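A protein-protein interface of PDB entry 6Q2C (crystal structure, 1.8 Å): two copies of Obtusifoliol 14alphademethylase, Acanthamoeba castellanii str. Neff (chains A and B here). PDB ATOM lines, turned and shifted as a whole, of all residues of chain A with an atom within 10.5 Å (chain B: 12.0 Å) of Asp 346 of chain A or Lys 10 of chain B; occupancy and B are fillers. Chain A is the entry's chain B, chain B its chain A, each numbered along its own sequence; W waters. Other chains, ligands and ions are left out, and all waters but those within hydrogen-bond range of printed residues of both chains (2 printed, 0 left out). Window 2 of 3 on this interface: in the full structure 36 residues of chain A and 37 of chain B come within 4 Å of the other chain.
Pro 12 of chain B touches Ile 46 of chain A (CG to CG1, 3.9 Å).
O of Ile 46 of chain A touches CD of Pro 13 of chain B, at 3.7 Å.
Phe 47 of chain A touches Pro 13 of chain B.
Thr 48 of chain A touches Val 14 of chain B (O to CA, 3.3 Å).
NH1 of Arg 55 of chain A touches CD1 of Leu 11 of chain B (3.97 Å).
Tyr 347 of chain A touches Lys 10 of chain B.
CD1 of Tyr 347 of chain A touches C of Leu 11 of chain B, at 3.9 Å.
Tyr 347 of chain A touches Pro 12 of chain B (CD1 to N, 3.8 Å).
Tyr 348 of chain A touches Leu 11 of chain B.
Tyr 348 of chain A touches Pro 12 of chain B.
No position is printed for both chains.
Of the 15 pairs that touch across the chains among the printed residues, none has its exchanged pair printed and touching as well.
The backbone carbonyl oxygen (O) of Lys 10 of chain B is in hydrogen-bond range of the backbone NH (N) of Tyr 348 of chain A, 2.9 Å away.
The side-chain amino group of Lys 10 of chain B is in salt-bridge range of the side-chain carboxylate of Asp 346 of chain A (2.9 Å).
O of Pro 13 of chain B sits at hydrogen-bond distance from N of Thr 48 of chain A.
OG1 of Thr 48 of chain A is in hydrogen-bond range of OG1 of Thr 57 of chain A, at 2.7 Å.
NE of Arg 55 of chain A lies within salt-bridge range of OD1 of Asp 353 of chain A, 2.8 Å away.
Of the 7 printed residues of chain B, 6 touch a printed residue of chain A.
Printed residues of chain B that touch a printed residue of chain A: Gly 9, Lys 10, Leu 11, Pro 12, Pro 13 and Val 14.
Hydrophobic or aromatic side chains of chain B within 4 Å of the printed part of chain A: Leu 11, Pro 12, Pro 13 and Val 14.
Along chain B the printed residues that touch a printed residue of chain A span positions 9 to 14.
Among the printed residues, Asp or Glu carboxylates within 4 Å of a Lys or Arg side-chain nitrogen of the other chain: Asp 346 of chain A with Lys 10 of chain B (2.9 Å).
Asp 346 of chain A touches just one residue of chain B: Lys 10.
No residue of chain B comes within 4 Å of Ser 343 of chain A.
No residue of chain B comes within 4 Å of Lys 345 of chain A.
Of chain A, only Arg 55 (3.97 Å), Tyr 347 (3.9 Å), Tyr 348 (3.7 Å) and Pro 350 (3.9 Å) come within 4 Å of Leu 11 of chain B.
Pro 12 of chain B touches just these residues of chain A: Ile 46 (3.9 Å), Tyr 347 (3.8 Å) and Tyr 348 (3.4 Å).
Printed residues of chain A within 4 Å of Pro 13 of chain B: Ile 46 (3.7 Å), Phe 47 (3.4 Å) and Thr 48 (2.8 Å).
Printed residues of chain A within 4 Å of Val 14 of chain B: Thr 48 (3.3 Å).
Of the printed residues of chain B, Thr 48 of chain A touches Pro 13 and Val 14.
Printed residues of chain B within 4 Å of Phe 47 of chain A: Pro 13.
Printed residues of chain B within 4 Å of Tyr 348 of chain A: Gly 9, Lys 10, Leu 11 and Pro 12.
Asp 45 of chain A touches none of the printed residues of chain B.
Pro 341 of chain A touches none of the printed residues of chain B.
The nearest residue of chain A that does not touch Lys 10 of chain B is Val 349 of chain A (5.5 Å).
The nearest printed residue of chain B that does not touch Tyr 348 of chain A is Lys 8 of chain B (4.1 Å).
Water W2 lies within hydrogen-bond range of the backbone carbonyl oxygen (O) of Asp 346 of chain A (2.6 Å) and the backbone NH (N) of Lys 10 of chain B (2.9 Å).
Water W1 lies within hydrogen-bond range of NH2 of Arg 55 of chain A (2.8 Å), O of Pro 12 of chain B (2.8 Å) and OG1 of Thr 48 of chain A (2.9 Å).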
ATOM      1  N   ASP A  45      36.366   0.242  22.320  1.00  0.00           N
ATOM      2  CA  ASP A  45      37.156  -0.716  23.070  1.00  0.00           C
ATOM      3  C   ASP A  45      36.634  -2.119  23.035  1.00  0.00           C
ATOM      4  O   ASP A  45      37.320  -3.055  23.466  1.00  0.00           O
ATOM      5  CB  ASP A  45      37.480  -0.214  24.491  1.00  0.00           C
ATOM      6  CG  ASP A  45      36.319  -0.184  25.424  1.00  0.00           C
ATOM      7  OD1 ASP A  45      35.172  -0.427  25.030  1.00  0.00           O
ATOM      8  OD2 ASP A  45      36.538   0.042  26.654  1.00  0.00           O
ATOM      9  N   ILE A  46      35.441  -2.286  22.472  1.00  0.00           N
ATOM     10  CA  ILE A  46      34.881  -3.601  22.235  1.00  0.00           C
ATOM     11  C   ILE A  46      34.259  -3.668  20.832  1.00  0.00           C
ATOM     12  O   ILE A  46      33.434  -2.782  20.474  1.00  0.00           O
ATOM     13  CB  ILE A  46      33.932  -4.001  23.340  1.00  0.00           C
ATOM     14  CG1 ILE A  46      33.324  -5.340  23.070  1.00  0.00           C
ATOM     15  CG2 ILE A  46      32.817  -2.988  23.546  1.00  0.00           C
ATOM     16  CD1 ILE A  46      32.606  -5.948  24.222  1.00  0.00           C
ATOM     17  N   PHE A  47      34.658  -4.664  20.017  1.00  0.00           N
ATOM     18  CA  PHE A  47      34.093  -4.802  18.654  1.00  0.00           C
ATOM     19  C   PHE A  47      34.304  -6.216  18.145  1.00  0.00           C
ATOM     20  O   PHE A  47      35.084  -6.945  18.708  1.00  0.00           O
ATOM     21  CB  PHE A  47      34.714  -3.785  17.692  1.00  0.00           C
ATOM     22  CG  PHE A  47      36.222  -3.878  17.594  1.00  0.00           C
ATOM     23  CD1 PHE A  47      36.834  -4.783  16.727  1.00  0.00           C
ATOM     24  CD2 PHE A  47      37.033  -3.145  18.436  1.00  0.00           C
ATOM     25  CE1 PHE A  47      38.208  -4.902  16.715  1.00  0.00           C
ATOM     26  CE2 PHE A  47      38.391  -3.236  18.397  1.00  0.00           C
ATOM     27  CZ  PHE A  47      38.996  -4.102  17.517  1.00  0.00           C
ATOM     28  N   THR A  48      33.621  -6.558  17.050  1.00  0.00           N
ATOM     29  CA  THR A  48      33.453  -7.917  16.637  1.00  0.00           C
ATOM     30  C   THR A  48      33.798  -8.004  15.154  1.00  0.00           C
ATOM     31  O   THR A  48      33.416  -7.133  14.357  1.00  0.00           O
ATOM     32  CB  THR A  48      32.056  -8.413  16.979  1.00  0.00           C
ATOM     33  OG1 THR A  48      31.817  -8.447  18.401  1.00  0.00           O
ATOM     34  CG2 THR A  48      31.809  -9.806  16.469  1.00  0.00           C
ATOM     35  N   ARG A  55      31.991 -15.437  15.402  1.00  0.00           N
ATOM     36  CA  ARG A  55      32.151 -14.097  15.941  1.00  0.00           C
ATOM     37  C   ARG A  55      33.414 -14.038  16.791  1.00  0.00           C
ATOM     38  O   ARG A  55      33.614 -14.867  17.683  1.00  0.00           O
ATOM     39  CB  ARG A  55      30.887 -13.746  16.771  1.00  0.00           C
ATOM     40  CG  ARG A  55      29.574 -13.433  15.966  1.00  0.00           C
ATOM     41  CD  ARG A  55      28.318 -13.450  16.850  1.00  0.00           C
ATOM     42  NE  ARG A  55      28.570 -12.586  17.994  1.00  0.00           N
ATOM     43  CZ  ARG A  55      28.579 -11.260  18.004  1.00  0.00           C
ATOM     44  NH1 ARG A  55      28.188 -10.517  16.949  1.00  0.00           N
ATOM     45  NH2 ARG A  55      28.976 -10.663  19.131  1.00  0.00           N
ATOM     46  N   THR A  57      35.404 -11.422  19.062  1.00  0.00           N
ATOM     47  CA  THR A  57      35.134 -10.164  19.790  1.00  0.00           C
ATOM     48  C   THR A  57      36.351  -9.675  20.514  1.00  0.00           C
ATOM     49  O   THR A  57      36.874 -10.364  21.387  1.00  0.00           O
ATOM     50  CB  THR A  57      33.928 -10.387  20.678  1.00  0.00           C
ATOM     51  OG1 THR A  57      32.758 -10.550  19.838  1.00  0.00           O
ATOM     52  CG2 THR A  57      33.694  -9.188  21.639  1.00  0.00           C
ATOM     53  N   PRO A 341      27.386 -15.830  28.977  1.00  0.00           N
ATOM     54  CA  PRO A 341      27.363 -14.471  28.406  1.00  0.00           C
ATOM     55  C   PRO A 341      27.670 -13.460  29.439  1.00  0.00           C
ATOM     56  O   PRO A 341      27.434 -13.707  30.601  1.00  0.00           O
ATOM     57  CB  PRO A 341      25.916 -14.286  27.900  1.00  0.00           C
ATOM     58  CG  PRO A 341      25.212 -15.559  28.214  1.00  0.00           C
ATOM     59  CD  PRO A 341      26.159 -16.595  28.706  1.00  0.00           C
ATOM     60  N   PHE A 342      28.186 -12.313  29.026  1.00  0.00           N
ATOM     61  CA  PHE A 342      28.462 -11.246  29.978  1.00  0.00           C
ATOM     62  C   PHE A 342      28.146  -9.931  29.353  1.00  0.00           C
ATOM     63  O   PHE A 342      28.040  -9.866  28.121  1.00  0.00           O
ATOM     64  CB  PHE A 342      29.957 -11.234  30.440  1.00  0.00           C
ATOM     65  CG  PHE A 342      30.964 -11.073  29.335  1.00  0.00           C
ATOM     66  CD1 PHE A 342      31.396  -9.839  28.950  1.00  0.00           C
ATOM     67  CD2 PHE A 342      31.505 -12.174  28.714  1.00  0.00           C
ATOM     68  CE1 PHE A 342      32.351  -9.654  27.971  1.00  0.00           C
ATOM     69  CE2 PHE A 342      32.445 -12.015  27.724  1.00  0.00           C
ATOM     70  CZ  PHE A 342      32.871 -10.784  27.331  1.00  0.00           C
ATOM     71  N   SER A 343      28.078  -8.898  30.216  1.00  0.00           N
ATOM     72  CA  SER A 343      27.900  -7.512  29.823  1.00  0.00           C
ATOM     73  C   SER A 343      29.132  -6.711  30.107  1.00  0.00           C
ATOM     74  O   SER A 343      29.840  -6.966  31.062  1.00  0.00           O
ATOM     75  CB  SER A 343      26.703  -6.892  30.600  1.00  0.00           C
ATOM     76  OG  SER A 343      25.528  -7.695  30.460  1.00  0.00           O
ATOM     77  N   TYR A 344      29.385  -5.740  29.257  1.00  0.00           N
ATOM     78  CA  TYR A 344      30.474  -4.865  29.370  1.00  0.00           C
ATOM     79  C   TYR A 344      29.889  -3.584  28.853  1.00  0.00           C
ATOM     80  O   TYR A 344      29.362  -3.570  27.722  1.00  0.00           O
ATOM     81  CB  TYR A 344      31.741  -5.324  28.543  1.00  0.00           C
ATOM     82  CG  TYR A 344      32.774  -4.222  28.524  1.00  0.00           C
ATOM     83  CD1 TYR A 344      33.380  -3.786  29.703  1.00  0.00           C
ATOM     84  CD2 TYR A 344      33.084  -3.545  27.395  1.00  0.00           C
ATOM     85  CE1 TYR A 344      34.247  -2.713  29.711  1.00  0.00           C
ATOM     86  CE2 TYR A 344      34.002  -2.517  27.403  1.00  0.00           C
ATOM     87  CZ  TYR A 344      34.595  -2.098  28.584  1.00  0.00           C
ATOM     88  OH  TYR A 344      35.517  -1.035  28.594  1.00  0.00           O
ATOM     89  N   LYS A 345      29.979  -2.509  29.652  1.00  0.00           N
ATOM     90  CA  LYS A 345      29.302  -1.219  29.358  1.00  0.00           C
ATOM     91  C   LYS A 345      27.840  -1.465  28.902  1.00  0.00           C
ATOM     92  O   LYS A 345      27.125  -2.226  29.573  1.00  0.00           O
ATOM     93  CB  LYS A 345      30.088  -0.373  28.362  1.00  0.00           C
ATOM     94  CG  LYS A 345      31.537  -0.075  28.711  1.00  0.00           C
ATOM     95  CD  LYS A 345      32.246   0.868  27.721  1.00  0.00           C
ATOM     96  CE  LYS A 345      31.888   0.558  26.243  1.00  0.00           C
ATOM     97  NZ  LYS A 345      32.730   1.133  25.123  1.00  0.00           N
ATOM     98  N   ASP A 346      27.379  -0.928  27.770  1.00  0.00           N
ATOM     99  CA  ASP A 346      25.954  -1.181  27.378  1.00  0.00           C
ATOM    100  C   ASP A 346      25.740  -2.474  26.550  1.00  0.00           C
ATOM    101  O   ASP A 346      24.621  -2.747  26.042  1.00  0.00           O
ATOM    102  CB  ASP A 346      25.339   0.053  26.652  1.00  0.00           C
ATOM    103  CG  ASP A 346      23.787   0.176  26.854  1.00  0.00           C
ATOM    104  OD1 ASP A 346      23.154  -0.698  27.518  1.00  0.00           O
ATOM    105  OD2 ASP A 346      23.187   1.148  26.320  1.00  0.00           O
ATOM    106  N   TYR A 347      26.769  -3.317  26.488  1.00  0.00           N
ATOM    107  CA  TYR A 347      26.816  -4.432  25.537  1.00  0.00           C
ATOM    108  C   TYR A 347      26.691  -5.799  26.143  1.00  0.00           C
ATOM    109  O   TYR A 347      26.961  -5.991  27.321  1.00  0.00           O
ATOM    110  CB  TYR A 347      28.094  -4.292  24.757  1.00  0.00           C
ATOM    111  CG  TYR A 347      28.171  -3.071  23.924  1.00  0.00           C
ATOM    112  CD1 TYR A 347      27.189  -2.811  22.914  1.00  0.00           C
ATOM    113  CD2 TYR A 347      29.237  -2.161  24.056  1.00  0.00           C
ATOM    114  CE1 TYR A 347      27.282  -1.696  22.082  1.00  0.00           C
ATOM    115  CE2 TYR A 347      29.346  -1.053  23.207  1.00  0.00           C
ATOM    116  CZ  TYR A 347      28.357  -0.836  22.229  1.00  0.00           C
ATOM    117  OH  TYR A 347      28.453   0.261  21.414  1.00  0.00           O
ATOM    118  N   TYR A 348      26.251  -6.758  25.322  1.00  0.00           N
ATOM    119  CA  TYR A 348      26.122  -8.128  25.671  1.00  0.00           C
ATOM    120  C   TYR A 348      27.044  -8.893  24.694  1.00  0.00           C
ATOM    121  O   TYR A 348      27.059  -8.599  23.472  1.00  0.00           O
ATOM    122  CB  TYR A 348      24.689  -8.531  25.420  1.00  0.00           C
ATOM    123  CG  TYR A 348      24.275  -9.938  25.687  1.00  0.00           C
ATOM    124  CD1 TYR A 348      23.991 -10.376  26.996  1.00  0.00           C
ATOM    125  CD2 TYR A 348      24.080 -10.823  24.642  1.00  0.00           C
ATOM    126  CE1 TYR A 348      23.534 -11.660  27.243  1.00  0.00           C
ATOM    127  CE2 TYR A 348      23.639 -12.110  24.860  1.00  0.00           C
ATOM    128  CZ  TYR A 348      23.367 -12.529  26.156  1.00  0.00           C
ATOM    129  OH  TYR A 348      22.961 -13.817  26.357  1.00  0.00           O
ATOM    130  N   VAL A 349      27.784  -9.854  25.253  1.00  0.00           N
ATOM    131  CA  VAL A 349      28.672 -10.770  24.507  1.00  0.00           C
ATOM    132  C   VAL A 349      28.100 -12.170  24.657  1.00  0.00           C
ATOM    133  O   VAL A 349      28.159 -12.763  25.738  1.00  0.00           O
ATOM    134  CB  VAL A 349      30.142 -10.711  24.998  1.00  0.00           C
ATOM    135  CG1 VAL A 349      31.002 -11.752  24.225  1.00  0.00           C
ATOM    136  CG2 VAL A 349      30.719  -9.309  24.813  1.00  0.00           C
ATOM    137  N   PRO A 350      27.536 -12.725  23.571  1.00  0.00           N
ATOM    138  CA  PRO A 350      26.856 -13.992  23.684  1.00  0.00           C
ATOM    139  C   PRO A 350      27.755 -15.195  23.842  1.00  0.00           C
ATOM    140  O   PRO A 350      28.933 -15.120  23.526  1.00  0.00           O
ATOM    141  CB  PRO A 350      26.047 -14.094  22.371  1.00  0.00           C
ATOM    142  CG  PRO A 350      26.659 -13.136  21.452  1.00  0.00           C
ATOM    143  CD  PRO A 350      27.494 -12.163  22.208  1.00  0.00           C
ATOM    144  N   ASP A 353      30.735 -16.710  21.359  1.00  0.00           N
ATOM    145  CA  ASP A 353      31.748 -15.834  20.830  1.00  0.00           C
ATOM    146  C   ASP A 353      33.156 -16.357  21.215  1.00  0.00           C
ATOM    147  O   ASP A 353      33.325 -17.079  22.208  1.00  0.00           O
ATOM    148  CB  ASP A 353      31.631 -14.413  21.392  1.00  0.00           C
ATOM    149  CG  ASP A 353      30.635 -13.531  20.622  1.00  0.00           C
ATOM    150  OD1 ASP A 353      29.633 -14.086  20.147  1.00  0.00           O
ATOM    151  OD2 ASP A 353      30.882 -12.309  20.553  1.00  0.00           O
ATOM    152  N   LYS B   8      19.562 -11.457  25.063  1.00  0.00           N
ATOM    153  CA  LYS B   8      19.031 -10.568  26.141  1.00  0.00           C
ATOM    154  C   LYS B   8      19.820  -9.236  26.295  1.00  0.00           C
ATOM    155  O   LYS B   8      20.109  -8.839  27.439  1.00  0.00           O
ATOM    156  CB  LYS B   8      18.988 -11.333  27.489  1.00  0.00           C
ATOM    157  N   GLY B   9      20.127  -8.542  25.169  1.00  0.00           N
ATOM    158  CA  GLY B   9      21.010  -7.335  25.173  1.00  0.00           C
ATOM    159  C   GLY B   9      21.543  -6.810  23.828  1.00  0.00           C
ATOM    160  O   GLY B   9      21.208  -7.336  22.782  1.00  0.00           O
ATOM    161  N   LYS B  10      22.347  -5.752  23.864  1.00  0.00           N
ATOM    162  CA  LYS B  10      22.929  -5.103  22.670  1.00  0.00           C
ATOM    163  C   LYS B  10      24.344  -5.582  22.152  1.00  0.00           C
ATOM    164  O   LYS B  10      25.311  -5.543  22.884  1.00  0.00           O
ATOM    165  CB  LYS B  10      23.025  -3.637  22.972  1.00  0.00           C
ATOM    166  CG  LYS B  10      21.661  -3.048  23.382  1.00  0.00           C
ATOM    167  CD  LYS B  10      21.780  -1.535  23.507  1.00  0.00           C
ATOM    168  CE  LYS B  10      20.669  -0.946  24.379  1.00  0.00           C
ATOM    169  NZ  LYS B  10      20.951   0.497  24.652  1.00  0.00           N
ATOM    170  N   LEU B  11      24.472  -5.948  20.873  1.00  0.00           N
ATOM    171  CA  LEU B  11      25.721  -6.522  20.393  1.00  0.00           C
ATOM    172  C   LEU B  11      26.627  -5.396  20.054  1.00  0.00           C
ATOM    173  O   LEU B  11      26.186  -4.406  19.466  1.00  0.00           O
ATOM    174  CB  LEU B  11      25.484  -7.419  19.174  1.00  0.00           C
ATOM    175  CG  LEU B  11      24.653  -8.642  19.402  1.00  0.00           C
ATOM    176  CD1 LEU B  11      24.545  -9.409  18.086  1.00  0.00           C
ATOM    177  CD2 LEU B  11      25.202  -9.550  20.466  1.00  0.00           C
ATOM    178  N   PRO B  12      27.933  -5.510  20.405  1.00  0.00           N
ATOM    179  CA  PRO B  12      28.916  -4.523  20.030  1.00  0.00           C
ATOM    180  C   PRO B  12      29.004  -4.397  18.555  1.00  0.00           C
ATOM    181  O   PRO B  12      28.532  -5.294  17.860  1.00  0.00           O
ATOM    182  CB  PRO B  12      30.249  -5.115  20.547  1.00  0.00           C
ATOM    183  CG  PRO B  12      29.927  -6.275  21.342  1.00  0.00           C
ATOM    184  CD  PRO B  12      28.504  -6.636  21.158  1.00  0.00           C
ATOM    185  N   PRO B  13      29.689  -3.387  18.064  1.00  0.00           N
ATOM    186  CA  PRO B  13      29.753  -3.175  16.634  1.00  0.00           C
ATOM    187  C   PRO B  13      30.478  -4.323  15.918  1.00  0.00           C
ATOM    188  O   PRO B  13      31.503  -4.789  16.395  1.00  0.00           O
ATOM    189  CB  PRO B  13      30.510  -1.837  16.471  1.00  0.00           C
ATOM    190  CG  PRO B  13      30.812  -1.371  17.813  1.00  0.00           C
ATOM    191  CD  PRO B  13      30.217  -2.251  18.820  1.00  0.00           C
ATOM    192  N   VAL B  14      29.854  -4.802  14.856  1.00  0.00           N
ATOM    193  CA  VAL B  14      30.431  -5.761  13.918  1.00  0.00           C
ATOM    194  C   VAL B  14      31.068  -4.990  12.802  1.00  0.00           C
ATOM    195  O   VAL B  14      30.376  -4.388  11.999  1.00  0.00           O
ATOM    196  CB  VAL B  14      29.348  -6.706  13.362  1.00  0.00           C
ATOM    197  CG1 VAL B  14      29.983  -7.744  12.433  1.00  0.00           C
ATOM    198  CG2 VAL B  14      28.654  -7.374  14.516  1.00  0.00           C
HETATM  199  O   HOH W   1      28.960  -8.095  18.138  1.00  0.00           O
HETATM  200  O   HOH W   2      23.187  -4.850  26.460  1.00  0.00           O
